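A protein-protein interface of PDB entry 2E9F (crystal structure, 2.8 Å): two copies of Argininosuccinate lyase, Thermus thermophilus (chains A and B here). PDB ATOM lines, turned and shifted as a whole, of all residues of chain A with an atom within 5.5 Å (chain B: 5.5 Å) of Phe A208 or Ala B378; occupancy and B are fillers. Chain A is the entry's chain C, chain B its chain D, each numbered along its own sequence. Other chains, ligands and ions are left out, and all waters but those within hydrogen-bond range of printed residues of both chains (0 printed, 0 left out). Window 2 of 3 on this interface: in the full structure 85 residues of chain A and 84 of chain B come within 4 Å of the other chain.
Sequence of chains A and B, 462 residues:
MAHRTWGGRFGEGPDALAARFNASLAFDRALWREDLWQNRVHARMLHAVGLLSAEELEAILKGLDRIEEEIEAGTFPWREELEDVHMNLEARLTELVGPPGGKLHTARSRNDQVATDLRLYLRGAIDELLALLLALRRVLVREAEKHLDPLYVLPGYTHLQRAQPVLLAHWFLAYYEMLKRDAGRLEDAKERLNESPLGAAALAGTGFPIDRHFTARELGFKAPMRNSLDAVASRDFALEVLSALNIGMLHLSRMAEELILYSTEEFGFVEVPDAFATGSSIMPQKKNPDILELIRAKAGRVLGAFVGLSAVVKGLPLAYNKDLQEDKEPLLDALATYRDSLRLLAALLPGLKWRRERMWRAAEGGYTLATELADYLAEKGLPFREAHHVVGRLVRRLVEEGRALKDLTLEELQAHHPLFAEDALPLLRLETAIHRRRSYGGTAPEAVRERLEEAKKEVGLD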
ATOM      1  N   LEU A  51      -3.497 -14.016  29.782  1.00  0.00           N
ATOM      2  CA  LEU A  51      -3.009 -15.200  29.073  1.00  0.00           C
ATOM      3  C   LEU A  51      -1.746 -15.821  29.681  1.00  0.00           C
ATOM      4  O   LEU A  51      -1.203 -16.789  29.144  1.00  0.00           O
ATOM      5  CB  LEU A  51      -2.761 -14.845  27.609  1.00  0.00           C
ATOM      6  CG  LEU A  51      -4.061 -14.504  26.886  1.00  0.00           C
ATOM      7  CD1 LEU A  51      -3.804 -13.952  25.486  1.00  0.00           C
ATOM      8  CD2 LEU A  51      -4.896 -15.775  26.831  1.00  0.00           C
ATOM      9  N   THR A 106       2.330 -16.436  22.182  1.00  0.00           N
ATOM     10  CA  THR A 106       0.881 -16.573  22.122  1.00  0.00           C
ATOM     11  C   THR A 106       0.302 -15.355  21.409  1.00  0.00           C
ATOM     12  O   THR A 106       0.782 -14.237  21.595  1.00  0.00           O
ATOM     13  CB  THR A 106       0.260 -16.634  23.525  1.00  0.00           C
ATOM     14  OG1 THR A 106       0.868 -17.689  24.278  1.00  0.00           O
ATOM     15  CG2 THR A 106      -1.233 -16.882  23.426  1.00  0.00           C
ATOM     16  N   ALA A 107      -0.717 -15.571  20.586  1.00  0.00           N
ATOM     17  CA  ALA A 107      -1.357 -14.476  19.869  1.00  0.00           C
ATOM     18  C   ALA A 107      -0.366 -13.501  19.219  1.00  0.00           C
ATOM     19  O   ALA A 107      -0.425 -12.291  19.461  1.00  0.00           O
ATOM     20  CB  ALA A 107      -2.280 -13.717  20.819  1.00  0.00           C
ATOM     21  N   THR A 206      -6.645 -10.751  16.107  1.00  0.00           N
ATOM     22  CA  THR A 206      -6.761 -12.002  16.840  1.00  0.00           C
ATOM     23  C   THR A 206      -8.066 -12.070  17.616  1.00  0.00           C
ATOM     24  O   THR A 206      -8.675 -11.038  17.943  1.00  0.00           O
ATOM     25  CB  THR A 206      -5.636 -12.187  17.871  1.00  0.00           C
ATOM     26  OG1 THR A 206      -4.654 -11.168  17.693  1.00  0.00           O
ATOM     27  CG2 THR A 206      -4.995 -13.540  17.709  1.00  0.00           C
ATOM     28  N   GLY A 207      -8.476 -13.302  17.911  1.00  0.00           N
ATOM     29  CA  GLY A 207      -9.682 -13.528  18.681  1.00  0.00           C
ATOM     30  C   GLY A 207      -9.268 -13.489  20.137  1.00  0.00           C
ATOM     31  O   GLY A 207     -10.098 -13.534  21.051  1.00  0.00           O
ATOM     32  N   PHE A 208      -7.956 -13.424  20.345  1.00  0.00           N
ATOM     33  CA  PHE A 208      -7.393 -13.360  21.684  1.00  0.00           C
ATOM     34  C   PHE A 208      -7.642 -11.986  22.278  1.00  0.00           C
ATOM     35  O   PHE A 208      -7.558 -10.966  21.589  1.00  0.00           O
ATOM     36  CB  PHE A 208      -5.883 -13.573  21.660  1.00  0.00           C
ATOM     37  CG  PHE A 208      -5.462 -14.982  21.417  1.00  0.00           C
ATOM     38  CD1 PHE A 208      -5.175 -15.424  20.133  1.00  0.00           C
ATOM     39  CD2 PHE A 208      -5.264 -15.849  22.482  1.00  0.00           C
ATOM     40  CE1 PHE A 208      -4.687 -16.703  19.908  1.00  0.00           C
ATOM     41  CE2 PHE A 208      -4.780 -17.125  22.265  1.00  0.00           C
ATOM     42  CZ  PHE A 208      -4.487 -17.553  20.971  1.00  0.00           C
ATOM     43  N   PRO A 209      -7.937 -11.936  23.574  1.00  0.00           N
ATOM     44  CA  PRO A 209      -8.186 -10.652  24.230  1.00  0.00           C
ATOM     45  C   PRO A 209      -6.910  -9.792  24.309  1.00  0.00           C
ATOM     46  O   PRO A 209      -6.594  -9.227  25.358  1.00  0.00           O
ATOM     47  CB  PRO A 209      -8.704 -11.075  25.600  1.00  0.00           C
ATOM     48  CG  PRO A 209      -7.967 -12.362  25.840  1.00  0.00           C
ATOM     49  CD  PRO A 209      -8.102 -13.054  24.514  1.00  0.00           C
ATOM     50  N   ILE A 210      -6.198  -9.692  23.189  1.00  0.00           N
ATOM     51  CA  ILE A 210      -4.949  -8.928  23.097  1.00  0.00           C
ATOM     52  C   ILE A 210      -5.137  -7.406  23.245  1.00  0.00           C
ATOM     53  O   ILE A 210      -6.106  -6.838  22.729  1.00  0.00           O
ATOM     54  CB  ILE A 210      -4.233  -9.276  21.745  1.00  0.00           C
ATOM     55  CG1 ILE A 210      -2.820  -9.782  22.025  1.00  0.00           C
ATOM     56  CG2 ILE A 210      -4.188  -8.080  20.803  1.00  0.00           C
ATOM     57  CD1 ILE A 210      -2.776 -11.070  22.819  1.00  0.00           C
ATOM     58  N   ALA B 374      -7.657 -23.516  16.958  1.00  0.00           N
ATOM     59  CA  ALA B 374      -6.478 -23.736  17.788  1.00  0.00           C
ATOM     60  C   ALA B 374      -6.268 -22.550  18.747  1.00  0.00           C
ATOM     61  O   ALA B 374      -5.838 -22.737  19.891  1.00  0.00           O
ATOM     62  CB  ALA B 374      -5.250 -23.952  16.905  1.00  0.00           C
ATOM     63  N   ASP B 375      -6.567 -21.334  18.281  1.00  0.00           N
ATOM     64  CA  ASP B 375      -6.436 -20.140  19.124  1.00  0.00           C
ATOM     65  C   ASP B 375      -7.376 -20.320  20.320  1.00  0.00           C
ATOM     66  O   ASP B 375      -7.089 -19.866  21.430  1.00  0.00           O
ATOM     67  CB  ASP B 375      -6.835 -18.868  18.359  1.00  0.00           C
ATOM     68  CG  ASP B 375      -5.717 -18.319  17.476  1.00  0.00           C
ATOM     69  OD1 ASP B 375      -5.927 -17.230  16.893  1.00  0.00           O
ATOM     70  OD2 ASP B 375      -4.645 -18.957  17.359  1.00  0.00           O
ATOM     71  N   TYR B 376      -8.505 -20.983  20.067  1.00  0.00           N
ATOM     72  CA  TYR B 376      -9.508 -21.269  21.091  1.00  0.00           C
ATOM     73  C   TYR B 376      -8.855 -22.094  22.203  1.00  0.00           C
ATOM     74  O   TYR B 376      -8.789 -21.665  23.355  1.00  0.00           O
ATOM     75  CB  TYR B 376     -10.672 -22.052  20.466  1.00  0.00           C
ATOM     76  CG  TYR B 376     -11.786 -22.420  21.425  1.00  0.00           C
ATOM     77  CD1 TYR B 376     -12.928 -21.623  21.549  1.00  0.00           C
ATOM     78  CD2 TYR B 376     -11.687 -23.558  22.233  1.00  0.00           C
ATOM     79  CE1 TYR B 376     -13.939 -21.951  22.456  1.00  0.00           C
ATOM     80  CE2 TYR B 376     -12.686 -23.892  23.138  1.00  0.00           C
ATOM     81  CZ  TYR B 376     -13.806 -23.087  23.247  1.00  0.00           C
ATOM     82  OH  TYR B 376     -14.776 -23.417  24.165  1.00  0.00           O
ATOM     83  N   LEU B 377      -8.355 -23.272  21.842  1.00  0.00           N
ATOM     84  CA  LEU B 377      -7.712 -24.152  22.807  1.00  0.00           C
ATOM     85  C   LEU B 377      -6.580 -23.470  23.560  1.00  0.00           C
ATOM     86  O   LEU B 377      -6.367 -23.736  24.743  1.00  0.00           O
ATOM     87  CB  LEU B 377      -7.177 -25.407  22.110  1.00  0.00           C
ATOM     88  CG  LEU B 377      -8.215 -26.380  21.542  1.00  0.00           C
ATOM     89  CD1 LEU B 377      -7.518 -27.634  21.054  1.00  0.00           C
ATOM     90  CD2 LEU B 377      -9.231 -26.747  22.618  1.00  0.00           C
ATOM     91  N   ALA B 378      -5.854 -22.592  22.870  1.00  0.00           N
ATOM     92  CA  ALA B 378      -4.721 -21.880  23.467  1.00  0.00           C
ATOM     93  C   ALA B 378      -5.173 -20.866  24.500  1.00  0.00           C
ATOM     94  O   ALA B 378      -4.525 -20.701  25.539  1.00  0.00           O
ATOM     95  CB  ALA B 378      -3.916 -21.181  22.388  1.00  0.00           C
ATOM     96  N   GLU B 379      -6.279 -20.186  24.191  1.00  0.00           N
ATOM     97  CA  GLU B 379      -6.868 -19.180  25.069  1.00  0.00           C
ATOM     98  C   GLU B 379      -7.377 -19.897  26.313  1.00  0.00           C
ATOM     99  O   GLU B 379      -7.319 -19.367  27.431  1.00  0.00           O
ATOM    100  CB  GLU B 379      -8.036 -18.480  24.363  1.00  0.00           C
ATOM    101  CG  GLU B 379      -8.399 -17.124  24.954  1.00  0.00           C
ATOM    102  CD  GLU B 379      -9.510 -16.429  24.191  1.00  0.00           C
ATOM    103  OE1 GLU B 379      -9.439 -16.396  22.936  1.00  0.00           O
ATOM    104  OE2 GLU B 379     -10.443 -15.908  24.848  1.00  0.00           O
ATOM    105  N   LYS B 380      -7.882 -21.113  26.106  1.00  0.00           N
ATOM    106  CA  LYS B 380      -8.389 -21.915  27.199  1.00  0.00           C
ATOM    107  C   LYS B 380      -7.254 -22.374  28.101  1.00  0.00           C
ATOM    108  O   LYS B 380      -7.411 -22.407  29.317  1.00  0.00           O
ATOM    109  CB  LYS B 380      -9.154 -23.118  26.663  1.00  0.00           C
ATOM    110  CG  LYS B 380     -10.600 -22.820  26.276  1.00  0.00           C
ATOM    111  CD  LYS B 380     -11.413 -22.368  27.481  1.00  0.00           C
ATOM    112  CE  LYS B 380     -12.885 -22.743  27.333  1.00  0.00           C
ATOM    113  NZ  LYS B 380     -13.115 -24.204  27.542  1.00  0.00           N
ATOM    114  N   GLY B 381      -6.107 -22.728  27.526  1.00  0.00           N
ATOM    115  CA  GLY B 381      -5.001 -23.159  28.362  1.00  0.00           C
ATOM    116  C   GLY B 381      -4.024 -24.141  27.749  1.00  0.00           C
ATOM    117  O   GLY B 381      -3.166 -24.683  28.439  1.00  0.00           O
ATOM    118  N   LEU B 382      -4.153 -24.383  26.455  1.00  0.00           N
ATOM    119  CA  LEU B 382      -3.242 -25.297  25.786  1.00  0.00           C
ATOM    120  C   LEU B 382      -2.078 -24.543  25.151  1.00  0.00           C
ATOM    121  O   LEU B 382      -2.294 -23.623  24.358  1.00  0.00           O
ATOM    122  CB  LEU B 382      -3.970 -26.077  24.694  1.00  0.00           C
ATOM    123  CG  LEU B 382      -4.205 -27.564  24.951  1.00  0.00           C
ATOM    124  CD1 LEU B 382      -4.473 -28.248  23.612  1.00  0.00           C
ATOM    125  CD2 LEU B 382      -2.986 -28.181  25.639  1.00  0.00           C
ATOM    126  N   PRO B 383      -0.829 -24.918  25.490  1.00  0.00           N
ATOM    127  CA  PRO B 383       0.333 -24.236  24.906  1.00  0.00           C
ATOM    128  C   PRO B 383       0.052 -24.054  23.411  1.00  0.00           C
ATOM    129  O   PRO B 383      -0.245 -25.031  22.715  1.00  0.00           O
ATOM    130  CB  PRO B 383       1.468 -25.216  25.182  1.00  0.00           C
ATOM    131  CG  PRO B 383       1.066 -25.810  26.499  1.00  0.00           C
ATOM    132  CD  PRO B 383      -0.408 -26.067  26.314  1.00  0.00           C
ATOM    133  N   PHE B 384       0.142 -22.815  22.921  1.00  0.00           N
ATOM    134  CA  PHE B 384      -0.182 -22.550  21.517  1.00  0.00           C
ATOM    135  C   PHE B 384       0.374 -23.589  20.547  1.00  0.00           C
ATOM    136  O   PHE B 384      -0.215 -23.846  19.492  1.00  0.00           O
ATOM    137  CB  PHE B 384       0.198 -21.101  21.114  1.00  0.00           C
ATOM    138  CG  PHE B 384       1.578 -20.941  20.529  1.00  0.00           C
ATOM    139  CD1 PHE B 384       2.612 -20.392  21.289  1.00  0.00           C
ATOM    140  CD2 PHE B 384       1.826 -21.265  19.197  1.00  0.00           C
ATOM    141  CE1 PHE B 384       3.878 -20.159  20.726  1.00  0.00           C
ATOM    142  CE2 PHE B 384       3.085 -21.038  18.628  1.00  0.00           C
ATOM    143  CZ  PHE B 384       4.113 -20.482  19.394  1.00  0.00           C
ATOM    144  N   ALA B 387      -1.725 -27.310  20.958  1.00  0.00           N
ATOM    145  CA  ALA B 387      -3.017 -27.101  20.307  1.00  0.00           C
ATOM    146  C   ALA B 387      -2.978 -27.306  18.791  1.00  0.00           C
ATOM    147  O   ALA B 387      -3.965 -27.735  18.190  1.00  0.00           O
ATOM    148  CB  ALA B 387      -3.529 -25.709  20.628  1.00  0.00           C
ATOM    149  N   ARG B 436     -14.386 -13.333  14.738  1.00  0.00           N
ATOM    150  CA  ARG B 436     -13.331 -13.705  15.662  1.00  0.00           C
ATOM    151  C   ARG B 436     -12.264 -12.631  15.895  1.00  0.00           C
ATOM    152  O   ARG B 436     -12.130 -12.119  17.011  1.00  0.00           O
ATOM    153  CB  ARG B 436     -12.670 -15.014  15.209  1.00  0.00           C
ATOM    154  CG  ARG B 436     -13.300 -16.267  15.816  1.00  0.00           C
ATOM    155  CD  ARG B 436     -13.106 -16.324  17.337  1.00  0.00           C
ATOM    156  NE  ARG B 436     -11.760 -16.721  17.762  1.00  0.00           N
ATOM    157  CZ  ARG B 436     -11.236 -16.439  18.958  1.00  0.00           C
ATOM    158  NH1 ARG B 436     -11.933 -15.749  19.856  1.00  0.00           N
ATOM    159  NH2 ARG B 436     -10.012 -16.851  19.273  1.00  0.00           N
ATOM    160  N   SER B 439      -9.831  -7.699  17.293  1.00  0.00           N
ATOM    161  CA  SER B 439      -8.826  -6.871  17.949  1.00  0.00           C
ATOM    162  C   SER B 439      -8.672  -5.577  17.152  1.00  0.00           C
ATOM    163  O   SER B 439      -9.108  -5.479  16.003  1.00  0.00           O
ATOM    164  CB  SER B 439      -7.495  -7.604  18.015  1.00  0.00           C
ATOM    165  OG  SER B 439      -7.097  -7.996  16.723  1.00  0.00           O
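OE1 of Glu B379 sits close to O of Gly A207, at 3.5 Å. OG of Ser B439 is in hydrogen-bond range of N of Thr A206 (2.9 Å). O of Gly A207 lies within hydrogen-bond range of NH1 of Arg B436, 3.1 Å away.
The side-chain carboxylate of Glu B379 lies within salt-bridge range of the guanidinium group of Arg B436 (3.7 Å).
Printed residues of chain B that touch a printed residue of chain A: Asp B375, Ala B378, Glu B379, Arg B436 and Ser B439. Along chain B the printed residues that touch a printed residue of chain A span positions 375 to 439. Of the 8 printed residues of chain A, 4 touch a printed residue of chain B. Among the printed residues, no Asp or Glu carboxylate lies within 4 Å of a Lys or Arg side-chain nitrogen of the other chain.
No position is printed for both chains.
Thr A206 touches Asp B375. Arg B436 touches Thr A206 (O to O, 3.7 Å). Phe A208 touches Asp B375. Ala B378 touches Phe A208 (CB to CZ, 3.9 Å). Phe A208 touches Glu B379. Pro A209 touches Glu B379.
Phe A208 touches just these residues of chain B: Asp B375, Ala B378 and Glu B379. Of the printed residues of chain A, Asp B375 touches Thr A206 (3.9 Å) and Phe A208 (3.1 Å). Of chain A, only Phe A208 comes within 4 Å of Ala B378. Printed residues of chain A within 4 Å of Glu B379: Gly A207, Phe A208 and Pro A209. The nearest residue of chain B that does not touch Phe A208 is Arg B436 (4.1 Å). The nearest residue of chain A that does not touch Ala B378 is Leu A51 (5.1 Å).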
